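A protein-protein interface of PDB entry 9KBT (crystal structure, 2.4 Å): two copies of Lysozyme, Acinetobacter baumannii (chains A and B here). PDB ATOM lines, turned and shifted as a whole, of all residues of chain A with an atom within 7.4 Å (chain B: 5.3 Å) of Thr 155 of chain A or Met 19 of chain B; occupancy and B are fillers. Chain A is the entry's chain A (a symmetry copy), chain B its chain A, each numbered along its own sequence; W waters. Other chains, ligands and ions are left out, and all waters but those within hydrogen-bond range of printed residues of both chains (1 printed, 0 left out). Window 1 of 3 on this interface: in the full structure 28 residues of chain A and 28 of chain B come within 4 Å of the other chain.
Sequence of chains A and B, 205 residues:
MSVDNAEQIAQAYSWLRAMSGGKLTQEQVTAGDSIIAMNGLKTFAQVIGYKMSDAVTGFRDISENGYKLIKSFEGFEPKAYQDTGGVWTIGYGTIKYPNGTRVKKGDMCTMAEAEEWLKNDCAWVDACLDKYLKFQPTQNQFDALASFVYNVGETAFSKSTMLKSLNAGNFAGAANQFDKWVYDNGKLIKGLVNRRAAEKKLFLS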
ATOM      1  N   TRP A  15      18.303  20.793  -1.171  1.00  0.00           N
ATOM      2  CA  TRP A  15      17.049  21.530  -1.165  1.00  0.00           C
ATOM      3  C   TRP A  15      15.871  20.572  -1.288  1.00  0.00           C
ATOM      4  O   TRP A  15      14.898  20.660  -0.527  1.00  0.00           O
ATOM      5  CB  TRP A  15      17.064  22.563  -2.289  1.00  0.00           C
ATOM      6  CG  TRP A  15      15.867  23.444  -2.320  1.00  0.00           C
ATOM      7  CD1 TRP A  15      15.733  24.671  -1.723  1.00  0.00           C
ATOM      8  CD2 TRP A  15      14.616  23.181  -2.986  1.00  0.00           C
ATOM      9  NE1 TRP A  15      14.478  25.181  -1.980  1.00  0.00           N
ATOM     10  CE2 TRP A  15      13.774  24.289  -2.751  1.00  0.00           C
ATOM     11  CE3 TRP A  15      14.128  22.119  -3.762  1.00  0.00           C
ATOM     12  CZ2 TRP A  15      12.471  24.367  -3.266  1.00  0.00           C
ATOM     13  CZ3 TRP A  15      12.821  22.195  -4.261  1.00  0.00           C
ATOM     14  CH2 TRP A  15      12.016  23.310  -4.011  1.00  0.00           C
ATOM     15  N   ALA A  18      15.132  18.725   1.989  1.00  0.00           N
ATOM     16  CA  ALA A  18      14.252  19.410   2.924  1.00  0.00           C
ATOM     17  C   ALA A  18      12.811  19.396   2.426  1.00  0.00           C
ATOM     18  O   ALA A  18      11.878  19.209   3.212  1.00  0.00           O
ATOM     19  CB  ALA A  18      14.735  20.838   3.153  1.00  0.00           C
ATOM     20  N   MET A  19      12.603  19.579   1.121  1.00  0.00           N
ATOM     21  CA  MET A  19      11.243  19.543   0.628  1.00  0.00           C
ATOM     22  C   MET A  19      10.643  18.161   0.725  1.00  0.00           C
ATOM     23  O   MET A  19       9.419  18.041   0.763  1.00  0.00           O
ATOM     24  CB  MET A  19      11.177  20.056  -0.802  1.00  0.00           C
ATOM     25  CG  MET A  19      11.613  21.524  -0.939  1.00  0.00           C
ATOM     26  SD  MET A  19      10.367  22.793  -0.494  1.00  0.00           S
ATOM     27  CE  MET A  19      10.336  22.748   1.317  1.00  0.00           C
ATOM     28  N   SER A  20      11.468  17.123   0.796  1.00  0.00           N
ATOM     29  CA  SER A  20      10.993  15.756   0.950  1.00  0.00           C
ATOM     30  C   SER A  20      10.936  15.324   2.408  1.00  0.00           C
ATOM     31  O   SER A  20      10.939  14.120   2.685  1.00  0.00           O
ATOM     32  CB  SER A  20      11.880  14.796   0.154  1.00  0.00           C
ATOM     33  OG  SER A  20      11.780  15.068  -1.229  1.00  0.00           O
ATOM     34  N   GLY A  21      10.935  16.273   3.344  1.00  0.00           N
ATOM     35  CA  GLY A  21      10.696  15.936   4.733  1.00  0.00           C
ATOM     36  C   GLY A  21      11.880  15.416   5.511  1.00  0.00           C
ATOM     37  O   GLY A  21      11.682  14.745   6.523  1.00  0.00           O
ATOM     38  N   ILE A  48      11.197  20.325  -9.724  1.00  0.00           N
ATOM     39  CA  ILE A  48      11.044  20.334  -8.273  1.00  0.00           C
ATOM     40  C   ILE A  48      10.760  21.721  -7.721  1.00  0.00           C
ATOM     41  O   ILE A  48      10.382  21.845  -6.547  1.00  0.00           O
ATOM     42  CB  ILE A  48      12.296  19.727  -7.603  1.00  0.00           C
ATOM     43  CG1 ILE A  48      13.534  20.580  -7.870  1.00  0.00           C
ATOM     44  CG2 ILE A  48      12.509  18.285  -8.069  1.00  0.00           C
ATOM     45  CD1 ILE A  48      14.780  20.080  -7.153  1.00  0.00           C
ATOM     46  N   GLY A  49      10.916  22.771  -8.529  1.00  0.00           N
ATOM     47  CA  GLY A  49      10.742  24.119  -8.037  1.00  0.00           C
ATOM     48  C   GLY A  49      11.986  24.732  -7.446  1.00  0.00           C
ATOM     49  O   GLY A  49      11.893  25.704  -6.683  1.00  0.00           O
ATOM     50  N   CYS A 128      17.901  31.676  -0.044  1.00  0.00           N
ATOM     51  CA  CYS A 128      16.543  31.448   0.418  1.00  0.00           C
ATOM     52  C   CYS A 128      16.215  32.373   1.582  1.00  0.00           C
ATOM     53  O   CYS A 128      15.181  33.054   1.576  1.00  0.00           O
ATOM     54  CB  CYS A 128      16.377  29.989   0.819  1.00  0.00           C
ATOM     55  SG  CYS A 128      14.736  29.584   1.367  1.00  0.00           S
ATOM     56  N   TYR A 132      12.900  35.686   1.819  1.00  0.00           N
ATOM     57  CA  TYR A 132      11.766  35.622   2.687  1.00  0.00           C
ATOM     58  C   TYR A 132      11.942  36.558   3.864  1.00  0.00           C
ATOM     59  O   TYR A 132      11.009  36.783   4.617  1.00  0.00           O
ATOM     60  CB  TYR A 132      11.565  34.207   3.164  1.00  0.00           C
ATOM     61  CG  TYR A 132      11.013  33.316   2.100  1.00  0.00           C
ATOM     62  CD1 TYR A 132       9.879  33.676   1.403  1.00  0.00           C
ATOM     63  CD2 TYR A 132      11.632  32.123   1.777  1.00  0.00           C
ATOM     64  CE1 TYR A 132       9.369  32.874   0.415  1.00  0.00           C
ATOM     65  CE2 TYR A 132      11.126  31.311   0.791  1.00  0.00           C
ATOM     66  CZ  TYR A 132       9.993  31.694   0.112  1.00  0.00           C
ATOM     67  OH  TYR A 132       9.464  30.901  -0.869  1.00  0.00           O
ATOM     68  N   VAL A 149      16.226  26.652   8.109  1.00  0.00           N
ATOM     69  CA  VAL A 149      15.721  26.497   6.748  1.00  0.00           C
ATOM     70  C   VAL A 149      16.380  25.298   6.063  1.00  0.00           C
ATOM     71  O   VAL A 149      15.726  24.543   5.333  1.00  0.00           O
ATOM     72  CB  VAL A 149      15.936  27.798   5.953  1.00  0.00           C
ATOM     73  CG1 VAL A 149      15.662  27.581   4.457  1.00  0.00           C
ATOM     74  CG2 VAL A 149      15.042  28.888   6.491  1.00  0.00           C
ATOM     75  N   VAL A 152      14.407  22.439   7.312  1.00  0.00           N
ATOM     76  CA  VAL A 152      12.963  22.399   7.202  1.00  0.00           C
ATOM     77  C   VAL A 152      12.472  22.728   5.800  1.00  0.00           C
ATOM     78  O   VAL A 152      11.385  22.273   5.419  1.00  0.00           O
ATOM     79  CB  VAL A 152      12.313  23.328   8.255  1.00  0.00           C
ATOM     80  CG1 VAL A 152      12.363  24.791   7.826  1.00  0.00           C
ATOM     81  CG2 VAL A 152      10.901  22.890   8.540  1.00  0.00           C
ATOM     82  N   GLY A 153      13.213  23.503   5.025  1.00  0.00           N
ATOM     83  CA  GLY A 153      12.944  23.645   3.612  1.00  0.00           C
ATOM     84  C   GLY A 153      12.245  24.946   3.271  1.00  0.00           C
ATOM     85  O   GLY A 153      11.582  25.572   4.098  1.00  0.00           O
ATOM     86  N   GLU A 154      12.385  25.335   1.998  1.00  0.00           N
ATOM     87  CA  GLU A 154      11.906  26.636   1.535  1.00  0.00           C
ATOM     88  C   GLU A 154      10.394  26.788   1.704  1.00  0.00           C
ATOM     89  O   GLU A 154       9.917  27.785   2.256  1.00  0.00           O
ATOM     90  CB  GLU A 154      12.299  26.851   0.077  1.00  0.00           C
ATOM     91  CG  GLU A 154      11.459  27.882  -0.587  1.00  0.00           C
ATOM     92  CD  GLU A 154      12.190  28.629  -1.648  1.00  0.00           C
ATOM     93  OE1 GLU A 154      13.312  28.210  -1.999  1.00  0.00           O
ATOM     94  OE2 GLU A 154      11.635  29.646  -2.127  1.00  0.00           O
ATOM     95  N   THR A 155       9.619  25.818   1.219  1.00  0.00           N
ATOM     96  CA  THR A 155       8.169  25.917   1.315  1.00  0.00           C
ATOM     97  C   THR A 155       7.726  25.977   2.773  1.00  0.00           C
ATOM     98  O   THR A 155       6.893  26.804   3.144  1.00  0.00           O
ATOM     99  CB  THR A 155       7.517  24.736   0.577  1.00  0.00           C
ATOM    100  OG1 THR A 155       7.600  24.939  -0.842  1.00  0.00           O
ATOM    101  CG2 THR A 155       6.062  24.595   0.946  1.00  0.00           C
ATOM    102  N   ALA A 156       8.307  25.128   3.622  1.00  0.00           N
ATOM    103  CA  ALA A 156       7.984  25.144   5.048  1.00  0.00           C
ATOM    104  C   ALA A 156       8.221  26.513   5.667  1.00  0.00           C
ATOM    105  O   ALA A 156       7.384  27.010   6.428  1.00  0.00           O
ATOM    106  CB  ALA A 156       8.805  24.093   5.791  1.00  0.00           C
ATOM    107  N   PHE A 157       9.356  27.135   5.362  1.00  0.00           N
ATOM    108  CA  PHE A 157       9.664  28.437   5.944  1.00  0.00           C
ATOM    109  C   PHE A 157       8.699  29.507   5.456  1.00  0.00           C
ATOM    110  O   PHE A 157       8.344  30.416   6.219  1.00  0.00           O
ATOM    111  CB  PHE A 157      11.106  28.819   5.610  1.00  0.00           C
ATOM    112  CG  PHE A 157      11.612  30.035   6.341  1.00  0.00           C
ATOM    113  CD1 PHE A 157      11.564  30.103   7.728  1.00  0.00           C
ATOM    114  CD2 PHE A 157      12.154  31.105   5.636  1.00  0.00           C
ATOM    115  CE1 PHE A 157      12.039  31.227   8.402  1.00  0.00           C
ATOM    116  CE2 PHE A 157      12.626  32.224   6.291  1.00  0.00           C
ATOM    117  CZ  PHE A 157      12.571  32.291   7.682  1.00  0.00           C
ATOM    118  N   SER A 158       8.242  29.399   4.205  1.00  0.00           N
ATOM    119  CA  SER A 158       7.389  30.425   3.615  1.00  0.00           C
ATOM    120  C   SER A 158       5.954  30.386   4.129  1.00  0.00           C
ATOM    121  O   SER A 158       5.221  31.362   3.946  1.00  0.00           O
ATOM    122  CB  SER A 158       7.381  30.274   2.107  1.00  0.00           C
ATOM    123  OG  SER A 158       6.645  29.130   1.743  1.00  0.00           O
ATOM    124  N   LYS A 159       5.532  29.276   4.738  1.00  0.00           N
ATOM    125  CA  LYS A 159       4.195  29.130   5.303  1.00  0.00           C
ATOM    126  C   LYS A 159       4.202  29.194   6.827  1.00  0.00           C
ATOM    127  O   LYS A 159       3.166  28.954   7.459  1.00  0.00           O
ATOM    128  CB  LYS A 159       3.553  27.805   4.868  1.00  0.00           C
ATOM    129  CG  LYS A 159       3.024  27.683   3.436  1.00  0.00           C
ATOM    130  CD  LYS A 159       3.773  28.493   2.416  1.00  0.00           C
ATOM    131  CE  LYS A 159       2.969  28.655   1.146  1.00  0.00           C
ATOM    132  NZ  LYS A 159       3.644  29.597   0.200  1.00  0.00           N
ATOM    133  N   SER A 160       5.347  29.485   7.432  1.00  0.00           N
ATOM    134  CA  SER A 160       5.489  29.329   8.870  1.00  0.00           C
ATOM    135  C   SER A 160       4.872  30.508   9.614  1.00  0.00           C
ATOM    136  O   SER A 160       5.038  31.667   9.221  1.00  0.00           O
ATOM    137  CB  SER A 160       6.968  29.189   9.232  1.00  0.00           C
ATOM    138  OG  SER A 160       7.712  30.266   8.692  1.00  0.00           O
ATOM    139  N   TRP A 181       8.327  22.934  16.142  1.00  0.00           N
ATOM    140  CA  TRP A 181       8.730  22.045  15.067  1.00  0.00           C
ATOM    141  C   TRP A 181       9.484  20.845  15.542  1.00  0.00           C
ATOM    142  O   TRP A 181      10.633  20.682  15.218  1.00  0.00           O
ATOM    143  CB  TRP A 181       9.619  22.805  14.105  1.00  0.00           C
ATOM    144  CG  TRP A 181       8.982  23.989  13.458  1.00  0.00           C
ATOM    145  CD1 TRP A 181       8.864  25.238  13.976  1.00  0.00           C
ATOM    146  CD2 TRP A 181       8.398  24.041  12.155  1.00  0.00           C
ATOM    147  NE1 TRP A 181       8.235  26.065  13.086  1.00  0.00           N
ATOM    148  CE2 TRP A 181       7.939  25.353  11.957  1.00  0.00           C
ATOM    149  CE3 TRP A 181       8.213  23.104  11.138  1.00  0.00           C
ATOM    150  CZ2 TRP A 181       7.311  25.752  10.786  1.00  0.00           C
ATOM    151  CZ3 TRP A 181       7.587  23.504   9.977  1.00  0.00           C
ATOM    152  CH2 TRP A 181       7.146  24.814   9.810  1.00  0.00           C
ATOM    153  N   TRP B  15      -0.472  16.809  -6.463  1.00  0.00           N
ATOM    154  CA  TRP B  15       0.354  16.531  -5.299  1.00  0.00           C
ATOM    155  C   TRP B  15       1.571  17.447  -5.283  1.00  0.00           C
ATOM    156  O   TRP B  15       1.892  18.061  -4.256  1.00  0.00           O
ATOM    157  CB  TRP B  15       0.750  15.057  -5.299  1.00  0.00           C
ATOM    158  CG  TRP B  15       1.520  14.634  -4.101  1.00  0.00           C
ATOM    159  CD1 TRP B  15       1.015  14.095  -2.946  1.00  0.00           C
ATOM    160  CD2 TRP B  15       2.949  14.707  -3.920  1.00  0.00           C
ATOM    161  NE1 TRP B  15       2.042  13.830  -2.065  1.00  0.00           N
ATOM    162  CE2 TRP B  15       3.236  14.195  -2.637  1.00  0.00           C
ATOM    163  CE3 TRP B  15       4.012  15.150  -4.720  1.00  0.00           C
ATOM    164  CZ2 TRP B  15       4.544  14.112  -2.135  1.00  0.00           C
ATOM    165  CZ3 TRP B  15       5.314  15.079  -4.209  1.00  0.00           C
ATOM    166  CH2 TRP B  15       5.562  14.563  -2.934  1.00  0.00           C
ATOM    167  N   LEU B  16       2.234  17.573  -6.433  1.00  0.00           N
ATOM    168  CA  LEU B  16       3.333  18.516  -6.582  1.00  0.00           C
ATOM    169  C   LEU B  16       2.879  19.940  -6.306  1.00  0.00           C
ATOM    170  O   LEU B  16       3.636  20.733  -5.732  1.00  0.00           O
ATOM    171  CB  LEU B  16       3.930  18.429  -7.995  1.00  0.00           C
ATOM    172  CG  LEU B  16       5.214  19.243  -8.203  1.00  0.00           C
ATOM    173  CD1 LEU B  16       6.275  18.805  -7.182  1.00  0.00           C
ATOM    174  CD2 LEU B  16       5.753  19.142  -9.624  1.00  0.00           C
ATOM    175  N   ARG B  17       1.659  20.290  -6.732  1.00  0.00           N
ATOM    176  CA  ARG B  17       1.157  21.643  -6.499  1.00  0.00           C
ATOM    177  C   ARG B  17       1.123  21.972  -5.011  1.00  0.00           C
ATOM    178  O   ARG B  17       1.481  23.085  -4.610  1.00  0.00           O
ATOM    179  CB  ARG B  17      -0.235  21.827  -7.098  1.00  0.00           C
ATOM    180  CG  ARG B  17      -0.896  23.168  -6.704  1.00  0.00           C
ATOM    181  CD  ARG B  17      -2.318  23.361  -7.278  1.00  0.00           C
ATOM    182  NE  ARG B  17      -3.342  22.581  -6.583  1.00  0.00           N
ATOM    183  CZ  ARG B  17      -4.649  22.826  -6.637  1.00  0.00           C
ATOM    184  NH1 ARG B  17      -5.141  23.817  -7.367  1.00  0.00           N
ATOM    185  NH2 ARG B  17      -5.485  22.062  -5.934  1.00  0.00           N
ATOM    186  N   ALA B  18       0.710  21.015  -4.176  1.00  0.00           N
ATOM    187  CA  ALA B  18       0.724  21.260  -2.742  1.00  0.00           C
ATOM    188  C   ALA B  18       2.152  21.288  -2.209  1.00  0.00           C
ATOM    189  O   ALA B  18       2.488  22.118  -1.358  1.00  0.00           O
ATOM    190  CB  ALA B  18      -0.107  20.206  -2.018  1.00  0.00           C
ATOM    191  N   MET B  19       3.017  20.399  -2.701  1.00  0.00           N
ATOM    192  CA  MET B  19       4.383  20.428  -2.225  1.00  0.00           C
ATOM    193  C   MET B  19       5.111  21.673  -2.673  1.00  0.00           C
ATOM    194  O   MET B  19       6.087  22.060  -2.031  1.00  0.00           O
ATOM    195  CB  MET B  19       5.132  19.181  -2.666  1.00  0.00           C
ATOM    196  CG  MET B  19       4.537  17.883  -2.094  1.00  0.00           C
ATOM    197  SD  MET B  19       4.990  17.468  -0.368  1.00  0.00           S
ATOM    198  CE  MET B  19       3.997  18.613   0.625  1.00  0.00           C
ATOM    199  N   SER B  20       4.648  22.323  -3.735  1.00  0.00           N
ATOM    200  CA  SER B  20       5.242  23.561  -4.214  1.00  0.00           C
ATOM    201  C   SER B  20       4.556  24.792  -3.638  1.00  0.00           C
ATOM    202  O   SER B  20       4.664  25.876  -4.220  1.00  0.00           O
ATOM    203  CB  SER B  20       5.204  23.609  -5.743  1.00  0.00           C
ATOM    204  OG  SER B  20       6.006  22.581  -6.286  1.00  0.00           O
ATOM    205  N   GLY B  21       3.815  24.641  -2.540  1.00  0.00           N
ATOM    206  CA  GLY B  21       3.291  25.797  -1.842  1.00  0.00           C
ATOM    207  C   GLY B  21       2.027  26.404  -2.400  1.00  0.00           C
ATOM    208  O   GLY B  21       1.759  27.576  -2.136  1.00  0.00           O
ATOM    209  N   VAL B 152      -2.562  21.597   1.447  1.00  0.00           N
ATOM    210  CA  VAL B 152      -1.346  21.883   2.180  1.00  0.00           C
ATOM    211  C   VAL B 152      -0.235  20.886   1.884  1.00  0.00           C
ATOM    212  O   VAL B 152       0.945  21.242   2.012  1.00  0.00           O
ATOM    213  CB  VAL B 152      -1.635  21.962   3.698  1.00  0.00           C
ATOM    214  CG1 VAL B 152      -1.757  20.576   4.325  1.00  0.00           C
ATOM    215  CG2 VAL B 152      -0.579  22.783   4.390  1.00  0.00           C
ATOM    216  N   GLY B 153      -0.555  19.659   1.506  1.00  0.00           N
ATOM    217  CA  GLY B 153       0.428  18.750   0.964  1.00  0.00           C
ATOM    218  C   GLY B 153       0.886  17.707   1.965  1.00  0.00           C
ATOM    219  O   GLY B 153       0.803  17.883   3.180  1.00  0.00           O
ATOM    220  N   GLU B 154       1.410  16.604   1.418  1.00  0.00           N
ATOM    221  CA  GLU B 154       1.763  15.439   2.226  1.00  0.00           C
ATOM    222  C   GLU B 154       2.833  15.763   3.270  1.00  0.00           C
ATOM    223  O   GLU B 154       2.675  15.448   4.454  1.00  0.00           O
ATOM    224  CB  GLU B 154       2.231  14.299   1.328  1.00  0.00           C
ATOM    225  CG  GLU B 154       3.044  13.297   2.066  1.00  0.00           C
ATOM    226  CD  GLU B 154       2.900  11.919   1.519  1.00  0.00           C
ATOM    227  OE1 GLU B 154       2.303  11.774   0.432  1.00  0.00           O
ATOM    228  OE2 GLU B 154       3.385  10.977   2.188  1.00  0.00           O
ATOM    229  N   THR B 155       3.938  16.378   2.849  1.00  0.00           N
ATOM    230  CA  THR B 155       5.011  16.683   3.786  1.00  0.00           C
ATOM    231  C   THR B 155       4.522  17.625   4.881  1.00  0.00           C
ATOM    232  O   THR B 155       4.788  17.408   6.063  1.00  0.00           O
ATOM    233  CB  THR B 155       6.209  17.277   3.027  1.00  0.00           C
ATOM    234  OG1 THR B 155       6.904  16.239   2.318  1.00  0.00           O
ATOM    235  CG2 THR B 155       7.185  17.933   3.972  1.00  0.00           C
ATOM    236  N   ALA B 156       3.769  18.660   4.504  1.00  0.00           N
ATOM    237  CA  ALA B 156       3.212  19.589   5.486  1.00  0.00           C
ATOM    238  C   ALA B 156       2.369  18.873   6.529  1.00  0.00           C
ATOM    239  O   ALA B 156       2.489  19.145   7.728  1.00  0.00           O
ATOM    240  CB  ALA B 156       2.374  20.659   4.791  1.00  0.00           C
HETATM  241  O   HOH W   1       8.251  22.306  -4.978  1.00  0.00           O
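The backbone carbonyl oxygen of Met 19 of chain B is in hydrogen-bond range of the side-chain hydroxyl of Thr 155 of chain A (3.5 Å). The side-chain hydroxyl of Thr 155 of chain B is in hydrogen-bond range of the backbone carbonyl oxygen of Met 19 of chain A (3.5 Å).
The side-chain sulfur (SD) of Met 19 of chain B lies within hydrogen-bond range of the side-chain hydroxyl (OG1) of Thr 155 of chain B (3.5 Å). The side-chain hydroxyl (OG) of Ser 158 of chain A lies close to the side-chain amino group (NZ) of Lys 159 of chain A, at 3.4 Å. The backbone carbonyl oxygen (O) of Thr 155 of chain A lies within hydrogen-bond range of the side-chain hydroxyl (OG) of Ser 158 of chain A (2.7 Å). SD of Met 19 of chain A lies within hydrogen-bond range of OG1 of Thr 155 of chain A.
Among the printed residues, pairs that only touch across the chains: Lys 159 of chain A with Gly 21 of chain B (3.6 Å).
Printed residues of chain B within 4 Å of Met 19 of chain A: Thr 155 (3.5 Å). Ser 20 of chain A touches none of the printed residues of chain B. Of chain B, only Met 19 comes within 4 Å of Thr 155 of chain A. No residue of chain A comes within 4 Å of Ala 18 of chain B. Printed residues of chain A within 4 Å of Gly 21 of chain B: Lys 159 (3.6 Å). Printed residues of chain A within 4 Å of Thr 155 of chain B: Met 19 (3.5 Å). The nearest printed residue of chain B that does not touch Lys 159 of chain A is Ser 20 of chain B (5.9 Å).
Along chain A the printed residues that touch a printed residue of chain B span positions 19 to 159. Among the printed residues, 3 pairs touch across the chains.
Met 19 of chain A touches Thr 155 of chain B, and with the chains exchanged Thr 155 of chain A touches Met 19 of chain B. Positions printed for both chains: 15, 18, 19, 20, 21, 152, 153, 154, 155 and 156. Of the 3 pairs that touch across the chains among the printed residues, 2 have their exchanged pair printed and touching as well.
Water W1 bridges OG of Ser 20 of chain B (2.6 Å) and O of Ile 48 of chain A (2.7 Å).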
